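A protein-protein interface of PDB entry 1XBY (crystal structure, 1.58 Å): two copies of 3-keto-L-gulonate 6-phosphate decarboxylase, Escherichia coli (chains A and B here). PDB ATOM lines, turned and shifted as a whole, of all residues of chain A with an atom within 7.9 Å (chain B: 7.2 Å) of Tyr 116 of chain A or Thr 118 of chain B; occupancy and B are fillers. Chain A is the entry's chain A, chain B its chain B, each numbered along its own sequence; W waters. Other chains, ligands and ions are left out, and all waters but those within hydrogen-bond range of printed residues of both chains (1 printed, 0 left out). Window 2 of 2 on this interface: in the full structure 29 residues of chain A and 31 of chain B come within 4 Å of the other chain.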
ATOM      1  N   ILE A  87      -2.263  13.598 -11.025  1.00  0.00           N
ATOM      2  CA  ILE A  87      -3.648  13.172 -10.891  1.00  0.00           C
ATOM      3  C   ILE A  87      -4.516  13.602 -12.094  1.00  0.00           C
ATOM      4  O   ILE A  87      -4.281  14.638 -12.742  1.00  0.00           O
ATOM      5  CB  ILE A  87      -4.245  13.634  -9.551  1.00  0.00           C
ATOM      6  CG1 ILE A  87      -5.536  12.857  -9.246  1.00  0.00           C
ATOM      7  CG2 ILE A  87      -4.583  15.114  -9.572  1.00  0.00           C
ATOM      8  CD1 ILE A  87      -5.320  11.359  -8.989  1.00  0.00           C
ATOM      9  N   CYS A  88      -5.463  12.743 -12.428  1.00  0.00           N
ATOM     10  CA  CYS A  88      -6.253  12.927 -13.654  1.00  0.00           C
ATOM     11  C   CYS A  88      -7.030  14.241 -13.756  1.00  0.00           C
ATOM     12  O   CYS A  88      -7.151  14.756 -14.863  1.00  0.00           O
ATOM     13  CB  CYS A  88      -7.183  11.758 -13.842  1.00  0.00           C
ATOM     14  SG  CYS A  88      -8.265  11.435 -12.424  1.00  0.00           S
ATOM     15  N   CYS A  89      -7.510  14.795 -12.650  1.00  0.00           N
ATOM     16  CA  CYS A  89      -8.285  16.050 -12.753  1.00  0.00           C
ATOM     17  C   CYS A  89      -7.423  17.288 -13.014  1.00  0.00           C
ATOM     18  O   CYS A  89      -7.956  18.336 -13.320  1.00  0.00           O
ATOM     19  CB  CYS A  89      -9.175  16.302 -11.570  1.00  0.00           C
ATOM     20  SG  CYS A  89      -8.266  16.539 -10.071  1.00  0.00           S
ATOM     21  N   ALA A  90      -6.110  17.191 -12.906  1.00  0.00           N
ATOM     22  CA  ALA A  90      -5.223  18.359 -13.091  1.00  0.00           C
ATOM     23  C   ALA A  90      -5.455  19.023 -14.450  1.00  0.00           C
ATOM     24  O   ALA A  90      -5.674  18.377 -15.474  1.00  0.00           O
ATOM     25  CB  ALA A  90      -3.780  17.954 -12.940  1.00  0.00           C
ATOM     26  N   ASP A 112      -2.332   9.420 -13.173  1.00  0.00           N
ATOM     27  CA  ASP A 112      -3.064   8.509 -12.309  1.00  0.00           C
ATOM     28  C   ASP A 112      -4.589   8.706 -12.402  1.00  0.00           C
ATOM     29  O   ASP A 112      -5.115   9.820 -12.271  1.00  0.00           O
ATOM     30  CB  ASP A 112      -2.593   8.639 -10.880  1.00  0.00           C
ATOM     31  CG  ASP A 112      -3.266   7.611  -9.980  1.00  0.00           C
ATOM     32  OD1 ASP A 112      -2.694   6.509  -9.782  1.00  0.00           O
ATOM     33  OD2 ASP A 112      -4.376   7.801  -9.480  1.00  0.00           O
ATOM     34  N   LEU A 113      -5.312   7.620 -12.693  1.00  0.00           N
ATOM     35  CA  LEU A 113      -6.702   7.738 -13.085  1.00  0.00           C
ATOM     36  C   LEU A 113      -7.652   7.440 -11.936  1.00  0.00           C
ATOM     37  O   LEU A 113      -8.781   6.981 -12.133  1.00  0.00           O
ATOM     38  CB  LEU A 113      -6.998   6.849 -14.308  1.00  0.00           C
ATOM     39  CG  LEU A 113      -6.114   7.053 -15.529  1.00  0.00           C
ATOM     40  CD1 LEU A 113      -6.492   6.030 -16.570  1.00  0.00           C
ATOM     41  CD2 LEU A 113      -6.225   8.441 -16.082  1.00  0.00           C
ATOM     42  N   THR A 114      -7.269   7.801 -10.734  1.00  0.00           N
ATOM     43  CA  THR A 114      -8.128   7.541  -9.608  1.00  0.00           C
ATOM     44  C   THR A 114      -9.256   8.560  -9.602  1.00  0.00           C
ATOM     45  O   THR A 114      -9.005   9.761  -9.640  1.00  0.00           O
ATOM     46  CB  THR A 114      -7.360   7.657  -8.289  1.00  0.00           C
ATOM     47  OG1 THR A 114      -6.300   6.675  -8.225  1.00  0.00           O
ATOM     48  CG2 THR A 114      -8.280   7.357  -7.159  1.00  0.00           C
ATOM     49  N   GLY A 115     -10.497   8.111  -9.449  1.00  0.00           N
ATOM     50  CA  GLY A 115     -11.607   9.051  -9.370  1.00  0.00           C
ATOM     51  C   GLY A 115     -12.161   9.470 -10.731  1.00  0.00           C
ATOM     52  O   GLY A 115     -12.145   8.704 -11.705  1.00  0.00           O
ATOM     53  N   TYR A 116     -12.644  10.705 -10.812  1.00  0.00           N
ATOM     54  CA  TYR A 116     -13.418  11.152 -11.968  1.00  0.00           C
ATOM     55  C   TYR A 116     -12.541  11.800 -13.053  1.00  0.00           C
ATOM     56  O   TYR A 116     -11.770  12.735 -12.798  1.00  0.00           O
ATOM     57  CB  TYR A 116     -14.514  12.121 -11.521  1.00  0.00           C
ATOM     58  CG  TYR A 116     -15.134  12.913 -12.669  1.00  0.00           C
ATOM     59  CD1 TYR A 116     -16.280  12.455 -13.328  1.00  0.00           C
ATOM     60  CD2 TYR A 116     -14.569  14.119 -13.085  1.00  0.00           C
ATOM     61  CE1 TYR A 116     -16.849  13.184 -14.383  1.00  0.00           C
ATOM     62  CE2 TYR A 116     -15.120  14.854 -14.151  1.00  0.00           C
ATOM     63  CZ  TYR A 116     -16.257  14.380 -14.787  1.00  0.00           C
ATOM     64  OH  TYR A 116     -16.785  15.119 -15.818  1.00  0.00           O
ATOM     65  N   TRP A 117     -12.660  11.281 -14.270  1.00  0.00           N
ATOM     66  CA  TRP A 117     -12.001  11.815 -15.455  1.00  0.00           C
ATOM     67  C   TRP A 117     -12.856  11.431 -16.678  1.00  0.00           C
ATOM     68  O   TRP A 117     -13.804  10.634 -16.568  1.00  0.00           O
ATOM     69  CB  TRP A 117     -10.588  11.267 -15.624  1.00  0.00           C
ATOM     70  CG  TRP A 117     -10.536   9.789 -15.586  1.00  0.00           C
ATOM     71  CD1 TRP A 117     -10.570   8.988 -14.461  1.00  0.00           C
ATOM     72  CD2 TRP A 117     -10.425   8.906 -16.702  1.00  0.00           C
ATOM     73  NE1 TRP A 117     -10.501   7.666 -14.826  1.00  0.00           N
ATOM     74  CE2 TRP A 117     -10.427   7.576 -16.193  1.00  0.00           C
ATOM     75  CE3 TRP A 117     -10.374   9.091 -18.079  1.00  0.00           C
ATOM     76  CZ2 TRP A 117     -10.335   6.441 -17.029  1.00  0.00           C
ATOM     77  CZ3 TRP A 117     -10.275   7.945 -18.926  1.00  0.00           C
ATOM     78  CH2 TRP A 117     -10.258   6.658 -18.385  1.00  0.00           C
ATOM     79  N   THR A 118     -12.528  12.019 -17.811  1.00  0.00           N
ATOM     80  CA  THR A 118     -13.319  11.830 -19.041  1.00  0.00           C
ATOM     81  C   THR A 118     -12.441  11.370 -20.182  1.00  0.00           C
ATOM     82  O   THR A 118     -11.199  11.580 -20.212  1.00  0.00           O
ATOM     83  CB  THR A 118     -14.032  13.144 -19.463  1.00  0.00           C
ATOM     84  OG1 THR A 118     -13.078  14.115 -19.878  1.00  0.00           O
ATOM     85  CG2 THR A 118     -14.855  13.764 -18.334  1.00  0.00           C
ATOM     86  N   TRP A 119     -13.100  10.777 -21.191  1.00  0.00           N
ATOM     87  CA  TRP A 119     -12.419  10.344 -22.387  1.00  0.00           C
ATOM     88  C   TRP A 119     -11.858  11.525 -23.171  1.00  0.00           C
ATOM     89  O   TRP A 119     -10.823  11.406 -23.797  1.00  0.00           O
ATOM     90  CB  TRP A 119     -13.358   9.421 -23.218  1.00  0.00           C
ATOM     91  CG  TRP A 119     -13.575   8.130 -22.509  1.00  0.00           C
ATOM     92  CD1 TRP A 119     -14.682   7.725 -21.858  1.00  0.00           C
ATOM     93  CD2 TRP A 119     -12.577   7.129 -22.256  1.00  0.00           C
ATOM     94  NE1 TRP A 119     -14.472   6.500 -21.275  1.00  0.00           N
ATOM     95  CE2 TRP A 119     -13.184   6.105 -21.516  1.00  0.00           C
ATOM     96  CE3 TRP A 119     -11.256   6.957 -22.655  1.00  0.00           C
ATOM     97  CZ2 TRP A 119     -12.487   4.961 -21.116  1.00  0.00           C
ATOM     98  CZ3 TRP A 119     -10.585   5.826 -22.287  1.00  0.00           C
ATOM     99  CH2 TRP A 119     -11.186   4.846 -21.513  1.00  0.00           C
ATOM    100  N   GLU A 120     -12.493  12.691 -23.071  1.00  0.00           N
ATOM    101  CA  GLU A 120     -11.946  13.884 -23.704  1.00  0.00           C
ATOM    102  C   GLU A 120     -10.608  14.278 -23.051  1.00  0.00           C
ATOM    103  O   GLU A 120      -9.672  14.652 -23.753  1.00  0.00           O
ATOM    104  CB  GLU A 120     -12.957  15.060 -23.657  1.00  0.00           C
ATOM    105  CG  GLU A 120     -14.389  14.703 -24.084  1.00  0.00           C
ATOM    106  CD  GLU A 120     -15.300  14.126 -22.976  1.00  0.00           C
ATOM    107  OE1 GLU A 120     -15.910  14.935 -22.204  1.00  0.00           O
ATOM    108  OE2 GLU A 120     -15.440  12.864 -22.902  1.00  0.00           O
ATOM    109  N   GLN A 121     -10.519  14.175 -21.724  1.00  0.00           N
ATOM    110  CA  GLN A 121      -9.254  14.431 -21.015  1.00  0.00           C
ATOM    111  C   GLN A 121      -8.177  13.434 -21.438  1.00  0.00           C
ATOM    112  O   GLN A 121      -7.020  13.793 -21.655  1.00  0.00           O
ATOM    113  CB  GLN A 121      -9.423  14.357 -19.499  1.00  0.00           C
ATOM    114  CG  GLN A 121     -10.129  15.494 -18.825  1.00  0.00           C
ATOM    115  CD  GLN A 121     -10.420  15.137 -17.368  1.00  0.00           C
ATOM    116  OE1 GLN A 121     -11.391  14.482 -17.096  1.00  0.00           O
ATOM    117  NE2 GLN A 121      -9.554  15.551 -16.453  1.00  0.00           N
ATOM    118  N   TRP A 125      -4.412  14.202 -22.882  1.00  0.00           N
ATOM    119  CA  TRP A 125      -3.132  13.683 -22.366  1.00  0.00           C
ATOM    120  C   TRP A 125      -2.277  13.113 -23.504  1.00  0.00           C
ATOM    121  O   TRP A 125      -1.053  13.364 -23.631  1.00  0.00           O
ATOM    122  CB  TRP A 125      -3.335  12.599 -21.269  1.00  0.00           C
ATOM    123  CG  TRP A 125      -4.164  13.038 -20.075  1.00  0.00           C
ATOM    124  CD1 TRP A 125      -4.167  14.279 -19.478  1.00  0.00           C
ATOM    125  CD2 TRP A 125      -5.147  12.269 -19.388  1.00  0.00           C
ATOM    126  NE1 TRP A 125      -5.085  14.301 -18.459  1.00  0.00           N
ATOM    127  CE2 TRP A 125      -5.706  13.084 -18.394  1.00  0.00           C
ATOM    128  CE3 TRP A 125      -5.591  10.945 -19.477  1.00  0.00           C
ATOM    129  CZ2 TRP A 125      -6.679  12.637 -17.543  1.00  0.00           C
ATOM    130  CZ3 TRP A 125      -6.581  10.530 -18.625  1.00  0.00           C
ATOM    131  CH2 TRP A 125      -7.105  11.358 -17.687  1.00  0.00           C
ATOM    132  N   CYS B  88     -10.792  17.532  -5.936  1.00  0.00           N
ATOM    133  CA  CYS B  88     -12.168  17.387  -6.456  1.00  0.00           C
ATOM    134  C   CYS B  88     -12.453  16.038  -7.161  1.00  0.00           C
ATOM    135  O   CYS B  88     -13.587  15.544  -7.057  1.00  0.00           O
ATOM    136  CB  CYS B  88     -12.542  18.540  -7.420  1.00  0.00           C
ATOM    137  SG  CYS B  88     -11.365  18.844  -8.703  1.00  0.00           S
ATOM    138  N   CYS B  89     -11.464  15.451  -7.824  1.00  0.00           N
ATOM    139  CA  CYS B  89     -11.752  14.237  -8.616  1.00  0.00           C
ATOM    140  C   CYS B  89     -11.882  12.985  -7.739  1.00  0.00           C
ATOM    141  O   CYS B  89     -12.334  11.928  -8.204  1.00  0.00           O
ATOM    142  CB  CYS B  89     -10.718  14.004  -9.708  1.00  0.00           C
ATOM    143  SG  CYS B  89      -9.071  13.653  -9.115  1.00  0.00           S
ATOM    144  N   ALA B  90     -11.497  13.081  -6.477  1.00  0.00           N
ATOM    145  CA  ALA B  90     -11.487  11.895  -5.611  1.00  0.00           C
ATOM    146  C   ALA B  90     -12.847  11.247  -5.525  1.00  0.00           C
ATOM    147  O   ALA B  90     -13.896  11.909  -5.450  1.00  0.00           O
ATOM    148  CB  ALA B  90     -10.984  12.231  -4.231  1.00  0.00           C
ATOM    149  N   ASP B  91     -12.816   9.917  -5.501  1.00  0.00           N
ATOM    150  CA  ASP B  91     -14.003   9.175  -5.195  1.00  0.00           C
ATOM    151  C   ASP B  91     -14.677   9.761  -3.966  1.00  0.00           C
ATOM    152  O   ASP B  91     -14.020  10.167  -2.980  1.00  0.00           O
ATOM    153  CB  ASP B  91     -13.635   7.704  -4.926  1.00  0.00           C
ATOM    154  CG  ASP B  91     -14.881   6.826  -4.722  1.00  0.00           C
ATOM    155  OD1 ASP B  91     -15.455   6.413  -5.756  1.00  0.00           O
ATOM    156  OD2 ASP B  91     -15.378   6.579  -3.615  1.00  0.00           O
ATOM    157  N   GLY B 115      -8.902  22.138 -11.471  1.00  0.00           N
ATOM    158  CA  GLY B 115      -9.060  21.232 -12.603  1.00  0.00           C
ATOM    159  C   GLY B 115     -10.488  20.805 -12.833  1.00  0.00           C
ATOM    160  O   GLY B 115     -11.438  21.513 -12.481  1.00  0.00           O
ATOM    161  N   TYR B 116     -10.642  19.619 -13.412  1.00  0.00           N
ATOM    162  CA  TYR B 116     -11.905  19.232 -13.999  1.00  0.00           C
ATOM    163  C   TYR B 116     -12.785  18.528 -12.979  1.00  0.00           C
ATOM    164  O   TYR B 116     -12.361  17.624 -12.237  1.00  0.00           O
ATOM    165  CB  TYR B 116     -11.658  18.347 -15.223  1.00  0.00           C
ATOM    166  N   TRP B 117     -14.173  19.061 -12.607  1.00  0.00           N
ATOM    167  CA  TRP B 117     -15.197  18.541 -11.668  1.00  0.00           C
ATOM    168  C   TRP B 117     -16.510  18.963 -12.257  1.00  0.00           C
ATOM    169  O   TRP B 117     -16.526  19.796 -13.160  1.00  0.00           O
ATOM    170  CB  TRP B 117     -15.005  19.111 -10.255  1.00  0.00           C
ATOM    171  CG  TRP B 117     -15.031  20.598 -10.191  1.00  0.00           C
ATOM    172  CD1 TRP B 117     -14.007  21.454 -10.476  1.00  0.00           C
ATOM    173  CD2 TRP B 117     -16.158  21.416  -9.855  1.00  0.00           C
ATOM    174  NE1 TRP B 117     -14.423  22.757 -10.308  1.00  0.00           N
ATOM    175  CE2 TRP B 117     -15.738  22.757  -9.922  1.00  0.00           C
ATOM    176  CE3 TRP B 117     -17.476  21.144  -9.450  1.00  0.00           C
ATOM    177  CZ2 TRP B 117     -16.609  23.832  -9.647  1.00  0.00           C
ATOM    178  CZ3 TRP B 117     -18.332  22.206  -9.162  1.00  0.00           C
ATOM    179  CH2 TRP B 117     -17.891  23.538  -9.271  1.00  0.00           C
ATOM    180  N   THR B 118     -17.587  18.394 -11.733  1.00  0.00           N
ATOM    181  CA  THR B 118     -18.942  18.630 -12.216  1.00  0.00           C
ATOM    182  C   THR B 118     -19.905  18.990 -11.096  1.00  0.00           C
ATOM    183  O   THR B 118     -19.668  18.715  -9.926  1.00  0.00           O
ATOM    184  CB  THR B 118     -19.483  17.352 -12.908  1.00  0.00           C
ATOM    185  OG1 THR B 118     -19.609  16.312 -11.944  1.00  0.00           O
ATOM    186  CG2 THR B 118     -18.519  16.800 -13.929  1.00  0.00           C
ATOM    187  N   TRP B 119     -21.036  19.597 -11.450  1.00  0.00           N
ATOM    188  CA  TRP B 119     -22.056  19.941 -10.460  1.00  0.00           C
ATOM    189  C   TRP B 119     -22.675  18.753  -9.763  1.00  0.00           C
ATOM    190  O   TRP B 119     -23.142  18.870  -8.638  1.00  0.00           O
ATOM    191  CB  TRP B 119     -23.154  20.792 -11.110  1.00  0.00           C
ATOM    192  CG  TRP B 119     -22.597  22.088 -11.561  1.00  0.00           C
ATOM    193  CD1 TRP B 119     -22.330  22.486 -12.840  1.00  0.00           C
ATOM    194  CD2 TRP B 119     -22.128  23.129 -10.708  1.00  0.00           C
ATOM    195  NE1 TRP B 119     -21.785  23.751 -12.828  1.00  0.00           N
ATOM    196  CE2 TRP B 119     -21.653  24.166 -11.526  1.00  0.00           C
ATOM    197  CE3 TRP B 119     -22.101  23.303  -9.324  1.00  0.00           C
ATOM    198  CZ2 TRP B 119     -21.129  25.348 -11.001  1.00  0.00           C
ATOM    199  CZ3 TRP B 119     -21.624  24.468  -8.803  1.00  0.00           C
ATOM    200  CH2 TRP B 119     -21.120  25.477  -9.633  1.00  0.00           C
ATOM    201  N   GLU B 120     -22.664  17.596 -10.414  1.00  0.00           N
ATOM    202  CA  GLU B 120     -23.170  16.376  -9.783  1.00  0.00           C
ATOM    203  C   GLU B 120     -22.244  15.986  -8.625  1.00  0.00           C
ATOM    204  O   GLU B 120     -22.695  15.630  -7.527  1.00  0.00           O
ATOM    205  CB  GLU B 120     -23.289  15.226 -10.819  1.00  0.00           C
ATOM    206  N   GLN B 121     -20.948  16.092  -8.871  1.00  0.00           N
ATOM    207  CA  GLN B 121     -19.960  15.856  -7.825  1.00  0.00           C
ATOM    208  C   GLN B 121     -20.116  16.826  -6.700  1.00  0.00           C
ATOM    209  O   GLN B 121     -20.032  16.455  -5.551  1.00  0.00           O
ATOM    210  CB  GLN B 121     -18.568  15.966  -8.386  1.00  0.00           C
ATOM    211  CG  GLN B 121     -18.123  14.705  -8.956  1.00  0.00           C
ATOM    212  CD  GLN B 121     -17.175  14.930 -10.051  1.00  0.00           C
ATOM    213  OE1 GLN B 121     -16.276  15.759  -9.940  1.00  0.00           O
ATOM    214  NE2 GLN B 121     -17.352  14.187 -11.139  1.00  0.00           N
ATOM    215  N   ALA B 122     -20.367  18.093  -7.023  1.00  0.00           N
ATOM    216  CA  ALA B 122     -20.590  19.095  -6.003  1.00  0.00           C
ATOM    217  C   ALA B 122     -21.785  18.764  -5.131  1.00  0.00           C
ATOM    218  O   ALA B 122     -21.748  18.927  -3.924  1.00  0.00           O
ATOM    219  CB  ALA B 122     -20.713  20.530  -6.618  1.00  0.00           C
ATOM    220  N   GLN B 123     -22.858  18.261  -5.738  1.00  0.00           N
ATOM    221  CA  GLN B 123     -23.984  17.811  -4.920  1.00  0.00           C
ATOM    222  C   GLN B 123     -23.635  16.659  -3.986  1.00  0.00           C
ATOM    223  O   GLN B 123     -24.081  16.664  -2.852  1.00  0.00           O
ATOM    224  CB  GLN B 123     -25.209  17.438  -5.792  1.00  0.00           C
ATOM    225  CG  GLN B 123     -26.439  17.044  -4.943  1.00  0.00           C
ATOM    226  CD  GLN B 123     -26.940  18.186  -4.112  1.00  0.00           C
ATOM    227  OE1 GLN B 123     -27.112  19.288  -4.639  1.00  0.00           O
ATOM    228  NE2 GLN B 123     -27.141  17.961  -2.817  1.00  0.00           N
ATOM    229  N   GLN B 124     -22.844  15.695  -4.458  1.00  0.00           N
ATOM    230  CA  GLN B 124     -22.346  14.616  -3.611  1.00  0.00           C
ATOM    231  C   GLN B 124     -21.559  15.129  -2.424  1.00  0.00           C
ATOM    232  O   GLN B 124     -21.753  14.667  -1.321  1.00  0.00           O
ATOM    233  CB  GLN B 124     -21.477  13.664  -4.413  1.00  0.00           C
ATOM    234  CG  GLN B 124     -22.214  12.827  -5.453  1.00  0.00           C
ATOM    235  CD  GLN B 124     -21.341  11.705  -5.922  1.00  0.00           C
ATOM    236  OE1 GLN B 124     -21.577  10.556  -5.560  1.00  0.00           O
ATOM    237  NE2 GLN B 124     -20.271  12.033  -6.646  1.00  0.00           N
ATOM    238  N   TRP B 125     -20.655  16.097  -2.641  1.00  0.00           N
ATOM    239  CA  TRP B 125     -19.922  16.695  -1.526  1.00  0.00           C
ATOM    240  C   TRP B 125     -20.850  17.259  -0.477  1.00  0.00           C
ATOM    241  O   TRP B 125     -20.663  17.012   0.715  1.00  0.00           O
ATOM    242  CB  TRP B 125     -18.911  17.786  -1.997  1.00  0.00           C
ATOM    243  CG  TRP B 125     -17.987  17.318  -3.058  1.00  0.00           C
ATOM    244  CD1 TRP B 125     -17.425  16.074  -3.174  1.00  0.00           C
ATOM    245  CD2 TRP B 125     -17.501  18.070  -4.161  1.00  0.00           C
ATOM    246  NE1 TRP B 125     -16.659  16.009  -4.308  1.00  0.00           N
ATOM    247  CE2 TRP B 125     -16.686  17.226  -4.923  1.00  0.00           C
ATOM    248  CE3 TRP B 125     -17.654  19.389  -4.579  1.00  0.00           C
ATOM    249  CZ2 TRP B 125     -16.044  17.633  -6.086  1.00  0.00           C
ATOM    250  CZ3 TRP B 125     -17.015  19.782  -5.729  1.00  0.00           C
ATOM    251  CH2 TRP B 125     -16.238  18.920  -6.476  1.00  0.00           C
HETATM  252  O   HOH W   1      -8.486  11.411  -7.294  1.00  0.00           O
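The backbone carbonyl oxygen (O) of Thr 114 of chain A is in hydrogen-bond range of the side-chain sulfur (SG) of Cys 88 of chain A (3.3 Å).
SG of Cys 88 of chain A sits at hydrogen-bond distance from O of Tyr 116 of chain A (3.8 Å).
The side-chain amide nitrogen of Gln 121 of chain A lies within hydrogen-bond range of the backbone carbonyl oxygen of Cys 88 of chain A, 3.0 Å away.
The side-chain carboxylate (OD2) of Asp 112 of chain A sits at hydrogen-bond distance from the side-chain hydroxyl (OG1) of Thr 114 of chain A, 2.6 Å away.
N of Thr 118 of chain A is in hydrogen-bond range of OE1 of Gln 121 of chain A (2.8 Å).
The side-chain hydroxyl of Thr 118 of chain B is in hydrogen-bond range of the side-chain amide nitrogen of Gln 121 of chain B.
The backbone carbonyl oxygen (O) of Cys 89 of chain A sits at hydrogen-bond distance from the backbone NH (N) of Tyr 116 of chain B.
N of Tyr 116 of chain A lies within hydrogen-bond range of O of Cys 89 of chain B (2.9 Å).
The side-chain sulfur (SG) of Cys 89 of chain B sits close to the side-chain sulfur (SG) of Cys 89 of chain A, at 3.1 Å.
Water W1 bridges the backbone carbonyl oxygen (O) of Thr 114 of chain A and the side-chain sulfur (SG) of Cys 89 of chain B.
Cys 89 of chain B touches its own counterpart, Cys 89 of chain A.
Cys 89 of chain A touches Gly 115 of chain B, and with the chains exchanged Gly 115 of chain A touches Cys 89 of chain B.
Cys 89 of chain A touches Tyr 116 of chain B, and with the chains exchanged Tyr 116 of chain A touches Cys 89 of chain B.
Tyr 116 of chain A touches Gln 121 of chain B, and with the chains exchanged Gln 121 of chain A touches Tyr 116 of chain B.
Of the 10 pairs that touch across the chains among the printed residues, 7 have their exchanged pair printed and touching as well.
Of the 15 printed residues of chain A, 6 touch a printed residue of chain B.
Printed residues of chain A that touch a printed residue of chain B: Ile 87, Cys 89, Thr 114, Gly 115, Tyr 116 and Gln 121.
Hydrophobic or aromatic side chains of chain A that line the printed part of chain B: Ile 87 and Tyr 116.
Printed residues of chain B that touch a printed residue of chain A: Cys 89, Gly 115, Tyr 116, Thr 118 and Gln 121.
Among the printed residues, 10 pairs touch across the chains.
Among the printed residues, no Asp or Glu carboxylate lies within 4 Å of a Lys or Arg side-chain nitrogen of the other chain.
Printed residues of chain B within 4 Å of Tyr 116 of chain A: Cys 89, Thr 118 and Gln 121.
Thr 118 of chain B touches just one residue of chain A: Tyr 116 (3.1 Å).
Of the printed residues of chain A, Cys 89 of chain B touches Ile 87 (3.6 Å), Cys 89 (3.1 Å), Thr 114 (3.9 Å), Gly 115 (3.2 Å) and Tyr 116 (2.9 Å).
Printed residues of chain B within 4 Å of Thr 114 of chain A: Cys 89.
Of the printed residues of chain B, Ile 87 of chain A touches Cys 89 (3.6 Å).
Of the printed residues of chain B, Gln 121 of chain A touches Tyr 116.
Of the printed residues of chain B, Gly 115 of chain A touches Cys 89.
Asp 112 of chain A touches none of the printed residues of chain B.
The nearest residue of chain A that does not touch Thr 118 of chain B is Thr 118 of chain A (6.5 Å).
Cys 89 of chain B touches Ile 87 of chain A.
CA of Gly 115 of chain B touches O of Cys 89 of chain A (3.2 Å).
O of Thr 114 of chain A touches SG of Cys 89 of chain B (3.9 Å).
O of Cys 89 of chain B touches CA of Gly 115 of chain A, at 3.2 Å.
Tyr 116 of chain A touches Thr 118 of chain B (OH to CG2, 3.1 Å).
Tyr 116 of chain A touches Gln 121 of chain B.
Gln 121 of chain A touches Tyr 116 of chain B.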
